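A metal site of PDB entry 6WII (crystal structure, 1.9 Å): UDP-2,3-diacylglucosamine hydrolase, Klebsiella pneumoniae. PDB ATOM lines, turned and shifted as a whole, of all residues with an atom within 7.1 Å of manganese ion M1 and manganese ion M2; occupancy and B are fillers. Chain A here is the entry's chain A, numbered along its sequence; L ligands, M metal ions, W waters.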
ATOM      1  N   ALA A   7      26.805  -7.606 -31.483  1.00  0.00           N
ATOM      2  CA  ALA A   7      26.426  -7.043 -30.186  1.00  0.00           C
ATOM      3  C   ALA A   7      26.671  -8.106 -29.128  1.00  0.00           C
ATOM      4  O   ALA A   7      26.884  -9.290 -29.432  1.00  0.00           O
ATOM      5  CB  ALA A   7      24.974  -6.583 -30.161  1.00  0.00           C
ATOM      6  N   ASP A   8      26.618  -7.675 -27.866  1.00  0.00           N
ATOM      7  CA  ASP A   8      26.591  -8.606 -26.752  1.00  0.00           C
ATOM      8  C   ASP A   8      27.818  -9.529 -26.740  1.00  0.00           C
ATOM      9  O   ASP A   8      27.710 -10.738 -26.501  1.00  0.00           O
ATOM     10  CB  ASP A   8      25.299  -9.409 -26.760  1.00  0.00           C
ATOM     11  CG  ASP A   8      24.093  -8.507 -26.655  1.00  0.00           C
ATOM     12  OD1 ASP A   8      23.978  -7.808 -25.625  1.00  0.00           O
ATOM     13  OD2 ASP A   8      23.299  -8.457 -27.600  1.00  0.00           O
ATOM     14  N   LEU A   9      28.977  -8.945 -26.995  1.00  0.00           N
ATOM     15  CA  LEU A   9      30.230  -9.663 -26.801  1.00  0.00           C
ATOM     16  C   LEU A   9      30.579  -9.783 -25.322  1.00  0.00           C
ATOM     17  O   LEU A   9      31.175 -10.791 -24.906  1.00  0.00           O
ATOM     18  CB  LEU A   9      31.361  -8.964 -27.551  1.00  0.00           C
ATOM     19  CG  LEU A   9      31.247  -9.076 -29.078  1.00  0.00           C
ATOM     20  CD1 LEU A   9      30.359  -7.994 -29.687  1.00  0.00           C
ATOM     21  CD2 LEU A   9      32.642  -9.007 -29.657  1.00  0.00           C
ATOM     22  N   HIS A  10      30.236  -8.773 -24.517  1.00  0.00           N
ATOM     23  CA  HIS A  10      30.559  -8.758 -23.082  1.00  0.00           C
ATOM     24  C   HIS A  10      32.028  -9.068 -22.831  1.00  0.00           C
ATOM     25  O   HIS A  10      32.386  -9.904 -21.980  1.00  0.00           O
ATOM     26  CB  HIS A  10      29.665  -9.733 -22.304  1.00  0.00           C
ATOM     27  CG  HIS A  10      28.200  -9.447 -22.455  1.00  0.00           C
ATOM     28  ND1 HIS A  10      27.491  -8.723 -21.528  1.00  0.00           N
ATOM     29  CD2 HIS A  10      27.328  -9.782 -23.431  1.00  0.00           C
ATOM     30  CE1 HIS A  10      26.231  -8.620 -21.922  1.00  0.00           C
ATOM     31  NE2 HIS A  10      26.113  -9.260 -23.073  1.00  0.00           N
ATOM     32  N   LEU A  39      26.180  -3.011 -31.745  1.00  0.00           N
ATOM     33  CA  LEU A  39      24.906  -2.601 -31.132  1.00  0.00           C
ATOM     34  C   LEU A  39      24.873  -2.835 -29.627  1.00  0.00           C
ATOM     35  O   LEU A  39      23.896  -3.375 -29.107  1.00  0.00           O
ATOM     36  CB  LEU A  39      23.748  -3.335 -31.817  1.00  0.00           C
ATOM     37  CG  LEU A  39      23.625  -3.152 -33.331  1.00  0.00           C
ATOM     38  CD1 LEU A  39      22.275  -3.712 -33.862  1.00  0.00           C
ATOM     39  CD2 LEU A  39      23.801  -1.679 -33.739  1.00  0.00           C
ATOM     40  N   GLY A  40      25.933  -2.446 -28.930  1.00  0.00           N
ATOM     41  CA  GLY A  40      25.913  -2.396 -27.480  1.00  0.00           C
ATOM     42  C   GLY A  40      26.426  -3.661 -26.816  1.00  0.00           C
ATOM     43  O   GLY A  40      26.471  -4.747 -27.407  1.00  0.00           O
ATOM     44  N   ASP A  41      26.816  -3.500 -25.552  1.00  0.00           N
ATOM     45  CA  ASP A  41      27.364  -4.591 -24.740  1.00  0.00           C
ATOM     46  C   ASP A  41      28.594  -5.170 -25.401  1.00  0.00           C
ATOM     47  O   ASP A  41      28.807  -6.387 -25.454  1.00  0.00           O
ATOM     48  CB  ASP A  41      26.313  -5.677 -24.459  1.00  0.00           C
ATOM     49  CG  ASP A  41      25.285  -5.233 -23.434  1.00  0.00           C
ATOM     50  OD1 ASP A  41      25.383  -4.072 -22.953  1.00  0.00           O
ATOM     51  OD2 ASP A  41      24.368  -6.029 -23.103  1.00  0.00           O
ATOM     52  N   GLU A  44      31.705  -6.099 -20.950  1.00  0.00           N
ATOM     53  CA  GLU A  44      30.916  -6.583 -19.825  1.00  0.00           C
ATOM     54  C   GLU A  44      30.656  -5.482 -18.810  1.00  0.00           C
ATOM     55  O   GLU A  44      29.638  -5.514 -18.087  1.00  0.00           O
ATOM     56  CB  GLU A  44      31.634  -7.764 -19.166  1.00  0.00           C
ATOM     57  CG  GLU A  44      31.018  -8.277 -17.842  1.00  0.00           C
ATOM     58  CD  GLU A  44      29.581  -8.745 -17.959  1.00  0.00           C
ATOM     59  OE1 GLU A  44      29.070  -8.925 -19.086  1.00  0.00           O
ATOM     60  OE2 GLU A  44      28.941  -8.944 -16.895  1.00  0.00           O
ATOM     61  N   GLY A  78      25.106  -0.264 -24.953  1.00  0.00           N
ATOM     62  CA  GLY A  78      24.292  -1.288 -24.338  1.00  0.00           C
ATOM     63  C   GLY A  78      23.982  -0.944 -22.889  1.00  0.00           C
ATOM     64  O   GLY A  78      24.357   0.105 -22.375  1.00  0.00           O
ATOM     65  N   ASN A  79      23.279  -1.860 -22.237  1.00  0.00           N
ATOM     66  CA  ASN A  79      22.999  -1.694 -20.803  1.00  0.00           C
ATOM     67  C   ASN A  79      24.255  -1.848 -19.959  1.00  0.00           C
ATOM     68  O   ASN A  79      24.313  -1.303 -18.852  1.00  0.00           O
ATOM     69  CB  ASN A  79      21.928  -2.674 -20.353  1.00  0.00           C
ATOM     70  CG  ASN A  79      22.311  -4.114 -20.635  1.00  0.00           C
ATOM     71  OD1 ASN A  79      22.373  -4.537 -21.779  1.00  0.00           O
ATOM     72  ND2 ASN A  79      22.549  -4.895 -19.569  1.00  0.00           N
ATOM     73  N   ARG A  80      25.258  -2.574 -20.446  1.00  0.00           N
ATOM     74  CA  ARG A  80      26.487  -2.752 -19.664  1.00  0.00           C
ATOM     75  C   ARG A  80      27.480  -1.629 -19.881  1.00  0.00           C
ATOM     76  O   ARG A  80      28.214  -1.273 -18.940  1.00  0.00           O
ATOM     77  CB  ARG A  80      27.176  -4.074 -20.011  1.00  0.00           C
ATOM     78  CG  ARG A  80      26.321  -5.301 -19.867  1.00  0.00           C
ATOM     79  CD  ARG A  80      25.806  -5.480 -18.448  1.00  0.00           C
ATOM     80  NE  ARG A  80      26.914  -5.775 -17.540  1.00  0.00           N
ATOM     81  CZ  ARG A  80      26.754  -6.135 -16.275  1.00  0.00           C
ATOM     82  NH1 ARG A  80      25.529  -6.265 -15.763  1.00  0.00           N
ATOM     83  NH2 ARG A  80      27.811  -6.387 -15.510  1.00  0.00           N
ATOM     84  N   HIS A 114      20.168  -1.162 -29.385  1.00  0.00           N
ATOM     85  CA  HIS A 114      20.646  -2.260 -28.554  1.00  0.00           C
ATOM     86  C   HIS A 114      19.538  -3.256 -28.268  1.00  0.00           C
ATOM     87  O   HIS A 114      19.751  -4.473 -28.322  1.00  0.00           O
ATOM     88  CB  HIS A 114      21.232  -1.747 -27.226  1.00  0.00           C
ATOM     89  CG  HIS A 114      21.717  -2.853 -26.359  1.00  0.00           C
ATOM     90  ND1 HIS A 114      22.662  -3.762 -26.772  1.00  0.00           N
ATOM     91  CD2 HIS A 114      21.356  -3.240 -25.104  1.00  0.00           C
ATOM     92  CE1 HIS A 114      22.889  -4.641 -25.805  1.00  0.00           C
ATOM     93  NE2 HIS A 114      22.100  -4.345 -24.788  1.00  0.00           N
ATOM     94  N   GLY A 115      18.344  -2.773 -27.953  1.00  0.00           N
ATOM     95  CA  GLY A 115      17.196  -3.628 -27.711  1.00  0.00           C
ATOM     96  C   GLY A 115      16.634  -3.567 -26.313  1.00  0.00           C
ATOM     97  O   GLY A 115      15.485  -3.976 -26.117  1.00  0.00           O
ATOM     98  N   ASP A 116      17.399  -3.074 -25.329  1.00  0.00           N
ATOM     99  CA  ASP A 116      16.881  -3.094 -23.960  1.00  0.00           C
ATOM    100  C   ASP A 116      15.681  -2.183 -23.804  1.00  0.00           C
ATOM    101  O   ASP A 116      14.807  -2.451 -22.960  1.00  0.00           O
ATOM    102  CB  ASP A 116      17.976  -2.712 -22.954  1.00  0.00           C
ATOM    103  CG  ASP A 116      18.555  -1.337 -23.205  1.00  0.00           C
ATOM    104  OD1 ASP A 116      18.916  -1.022 -24.359  1.00  0.00           O
ATOM    105  OD2 ASP A 116      18.641  -0.554 -22.246  1.00  0.00           O
ATOM    106  N   TYR A 125      13.861  -2.553 -14.495  1.00  0.00           N
ATOM    107  CA  TYR A 125      15.043  -2.218 -15.281  1.00  0.00           C
ATOM    108  C   TYR A 125      14.914  -0.842 -15.913  1.00  0.00           C
ATOM    109  O   TYR A 125      15.873  -0.062 -15.899  1.00  0.00           O
ATOM    110  CB  TYR A 125      15.300  -3.254 -16.380  1.00  0.00           C
ATOM    111  CG  TYR A 125      16.326  -2.723 -17.355  1.00  0.00           C
ATOM    112  CD1 TYR A 125      17.621  -2.492 -16.942  1.00  0.00           C
ATOM    113  CD2 TYR A 125      15.983  -2.372 -18.650  1.00  0.00           C
ATOM    114  CE1 TYR A 125      18.572  -1.975 -17.804  1.00  0.00           C
ATOM    115  CE2 TYR A 125      16.927  -1.851 -19.524  1.00  0.00           C
ATOM    116  CZ  TYR A 125      18.214  -1.664 -19.089  1.00  0.00           C
ATOM    117  OH  TYR A 125      19.167  -1.143 -19.942  1.00  0.00           O
ATOM    118  N   ILE A 171      17.307 -12.955 -19.145  1.00  0.00           N
ATOM    119  CA  ILE A 171      17.076 -11.637 -19.717  1.00  0.00           C
ATOM    120  C   ILE A 171      15.630 -11.560 -20.170  1.00  0.00           C
ATOM    121  O   ILE A 171      15.163 -12.414 -20.944  1.00  0.00           O
ATOM    122  CB  ILE A 171      18.045 -11.354 -20.881  1.00  0.00           C
ATOM    123  CG1 ILE A 171      19.495 -11.423 -20.410  1.00  0.00           C
ATOM    124  CG2 ILE A 171      17.751  -9.996 -21.512  1.00  0.00           C
ATOM    125  CD1 ILE A 171      20.515 -11.372 -21.535  1.00  0.00           C
ATOM    126  N   GLY A 194      20.149  -6.373 -30.382  1.00  0.00           N
ATOM    127  CA  GLY A 194      20.702  -7.426 -29.576  1.00  0.00           C
ATOM    128  C   GLY A 194      20.018  -7.460 -28.231  1.00  0.00           C
ATOM    129  O   GLY A 194      18.784  -7.473 -28.163  1.00  0.00           O
ATOM    130  N   HIS A 195      20.832  -7.473 -27.173  1.00  0.00           N
ATOM    131  CA  HIS A 195      20.391  -7.452 -25.772  1.00  0.00           C
ATOM    132  C   HIS A 195      19.744  -8.738 -25.289  1.00  0.00           C
ATOM    133  O   HIS A 195      20.091  -9.214 -24.196  1.00  0.00           O
ATOM    134  CB  HIS A 195      19.393  -6.324 -25.470  1.00  0.00           C
ATOM    135  CG  HIS A 195      19.087  -6.233 -24.007  1.00  0.00           C
ATOM    136  ND1 HIS A 195      20.038  -5.904 -23.069  1.00  0.00           N
ATOM    137  CD2 HIS A 195      17.958  -6.520 -23.300  1.00  0.00           C
ATOM    138  CE1 HIS A 195      19.506  -5.937 -21.858  1.00  0.00           C
ATOM    139  NE2 HIS A 195      18.244  -6.323 -21.973  1.00  0.00           N
ATOM    140  N   THR A 196      18.787  -9.290 -26.035  1.00  0.00           N
ATOM    141  CA  THR A 196      18.002 -10.390 -25.482  1.00  0.00           C
ATOM    142  C   THR A 196      18.686 -11.737 -25.581  1.00  0.00           C
ATOM    143  O   THR A 196      18.190 -12.696 -25.000  1.00  0.00           O
ATOM    144  CB  THR A 196      16.641 -10.476 -26.171  1.00  0.00           C
ATOM    145  OG1 THR A 196      16.845 -10.727 -27.560  1.00  0.00           O
ATOM    146  CG2 THR A 196      15.863  -9.171 -25.975  1.00  0.00           C
ATOM    147  N   HIS A 197      19.795 -11.842 -26.330  1.00  0.00           N
ATOM    148  CA  HIS A 197      20.555 -13.088 -26.425  1.00  0.00           C
ATOM    149  C   HIS A 197      19.738 -14.236 -27.020  1.00  0.00           C
ATOM    150  O   HIS A 197      19.989 -15.399 -26.726  1.00  0.00           O
ATOM    151  CB  HIS A 197      21.113 -13.502 -25.060  1.00  0.00           C
ATOM    152  CG  HIS A 197      22.101 -12.541 -24.485  1.00  0.00           C
ATOM    153  ND1 HIS A 197      22.927 -12.865 -23.422  1.00  0.00           N
ATOM    154  CD2 HIS A 197      22.406 -11.259 -24.823  1.00  0.00           C
ATOM    155  CE1 HIS A 197      23.695 -11.824 -23.137  1.00  0.00           C
ATOM    156  NE2 HIS A 197      23.388 -10.835 -23.968  1.00  0.00           N
ATOM    157  N   ALA A 218      24.533 -13.440 -28.373  1.00  0.00           N
ATOM    158  CA  ALA A 218      25.671 -13.125 -27.526  1.00  0.00           C
ATOM    159  C   ALA A 218      26.826 -14.047 -27.890  1.00  0.00           C
ATOM    160  O   ALA A 218      26.627 -15.153 -28.396  1.00  0.00           O
ATOM    161  CB  ALA A 218      25.301 -13.288 -26.046  1.00  0.00           C
HETATM  162  C1  LIG L   1      26.557  -2.311 -15.821  1.00  0.00           C
HETATM  163  C2  LIG L   1      24.690  -3.330 -14.705  1.00  0.00           C
HETATM  164  C3  LIG L   1      26.721  -2.921 -13.494  1.00  0.00           C
HETATM  165  C4  LIG L   1      20.219  -4.763 -16.755  1.00  0.00           C
HETATM  166  C5  LIG L   1      19.162  -6.580 -18.147  1.00  0.00           C
HETATM  167  C6  LIG L   1      16.786  -6.540 -18.914  1.00  0.00           C
HETATM  168  C7  LIG L   1      26.876   4.324 -13.388  1.00  0.00           C
HETATM  169  C8  LIG L   1      27.110   3.279 -12.538  1.00  0.00           C
HETATM  170  C9  LIG L   1      28.492   1.259 -12.093  1.00  0.00           C
HETATM  171  C10 LIG L   1      28.328  -0.148 -12.637  1.00  0.00           C
HETATM  172  C11 LIG L   1      28.231   0.732 -14.901  1.00  0.00           C
HETATM  173  C12 LIG L   1      28.395   2.139 -14.356  1.00  0.00           C
HETATM  174  C13 LIG L   1      27.280  -2.382 -14.649  1.00  0.00           C
HETATM  175  C14 LIG L   1      25.268  -2.800 -15.849  1.00  0.00           C
HETATM  176  C15 LIG L   1      25.416  -3.372 -13.524  1.00  0.00           C
HETATM  177  C16 LIG L   1      22.422  -4.017 -15.837  1.00  0.00           C
HETATM  178  C17 LIG L   1      19.642  -6.182 -16.742  1.00  0.00           C
HETATM  179  C18 LIG L   1      17.995  -5.686 -18.552  1.00  0.00           C
HETATM  180  C19 LIG L   1      26.689   3.285 -11.213  1.00  0.00           C
HETATM  181  C20 LIG L   1      26.001   4.371 -10.758  1.00  0.00           C
HETATM  182  C21 LIG L   1      25.740   5.442 -11.592  1.00  0.00           C
HETATM  183  C22 LIG L   1      26.174   5.411 -12.908  1.00  0.00           C
HETATM  184  C23 LIG L   1      25.547   4.368  -9.299  1.00  0.00           C
HETATM  185  F1  LIG L   1      26.635   4.298  -8.500  1.00  0.00           F
HETATM  186  F2  LIG L   1      24.769   3.276  -9.087  1.00  0.00           F
HETATM  187  F3  LIG L   1      24.870   5.512  -9.041  1.00  0.00           F
HETATM  188  N1  LIG L   1      27.841   2.150 -13.016  1.00  0.00           N
HETATM  189  N2  LIG L   1      28.866  -0.199 -14.001  1.00  0.00           N
HETATM  190  N3  LIG L   1      23.350  -3.880 -14.693  1.00  0.00           N
HETATM  191  N4  LIG L   1      21.125  -4.621 -15.631  1.00  0.00           N
HETATM  192  N5  LIG L   1      16.069  -6.286 -20.148  1.00  0.00           N
HETATM  193  O1  LIG L   1      29.548  -1.617 -15.963  1.00  0.00           O
HETATM  194  O2  LIG L   1      29.807  -2.595 -13.792  1.00  0.00           O
HETATM  195  O3  LIG L   1      22.672  -3.645 -16.926  1.00  0.00           O
HETATM  196  O4  LIG L   1      16.428  -7.412 -18.190  1.00  0.00           O
HETATM  197  O5  LIG L   1      14.959  -7.081 -20.492  1.00  0.00           O
HETATM  198  S1  LIG L   1      28.956  -1.747 -14.628  1.00  0.00           S
HETATM  199 CL1  LIG L   1      25.871   6.735 -14.049  1.00  0.00          CL
HETATM  200 MN    MN M   1      24.088  -8.616 -23.767  1.00  0.00          MN
HETATM  201 MN    MN M   2      22.197  -5.863 -23.154  1.00  0.00          MN
HETATM  202  O   HOH W   1      23.127  -7.729 -20.436  1.00  0.00           O
HETATM  203  O   HOH W   2      22.523  -7.984 -22.944  1.00  0.00           O
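An oxygen (O3) of the ligand lies within hydrogen-bond range of the side-chain amide nitrogen (ND2) of Asn 79, at 2.9 Å. A ring nitrogen (NE2) of His 195 sits at hydrogen-bond distance from a nitrogen (N5) of the ligand (2.8 Å).
N of His 195 sits at hydrogen-bond distance from OD2 of Asp 8, at 2.7 Å. N of Asp 8 lies within hydrogen-bond range of O of Gly 40 (3.0 Å). The side-chain carboxylate (OD1) of Asp 41 is in hydrogen-bond range of the backbone NH (N) of Arg 80 (2.9 Å). O of Asp 41 lies within hydrogen-bond range of N of Leu 9 (3.0 Å). N of Gly 194 lies within hydrogen-bond range of O of His 114. The backbone carbonyl oxygen (O) of Leu 39 lies within hydrogen-bond range of a ring nitrogen (ND1) of His 114, 2.7 Å away. A ring nitrogen (ND1) of His 10 sits at hydrogen-bond distance from the side-chain carboxylate (OE1) of Glu 44 (2.9 Å).
Of the 21 residues printed, 4 come within 4 Å of manganese ion M1.
Of the 21 residues printed, 5 come within 4 Å of manganese ion M2. The nearest printed residue that does not touch manganese ion M2 is His 10 (5.0 Å).
Manganese ion M1 is bound by water W2, at 1.9 Å. The side-chain carboxylate (OD1) of Asp 8 binds manganese ion M1 (2.0 Å). Manganese ion M1 is bound by NE2 of His 10 (2.2 Å). Manganese ion M1 is bound by NE2 of His 197, 2.3 Å away. OD2 of Asp 41 is bound to manganese ion M1, 2.7 Å away.
Manganese ion M2 is bound by the side-chain amide oxygen (OD1) of Asn 79 (1.9 Å), water W2 (2.2 Å), a ring nitrogen (ND1) of His 195 (2.2 Å), the side-chain carboxylate (OD2) of Asp 41 (2.2 Å) and a ring nitrogen (NE2) of His 114 (2.2 Å).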
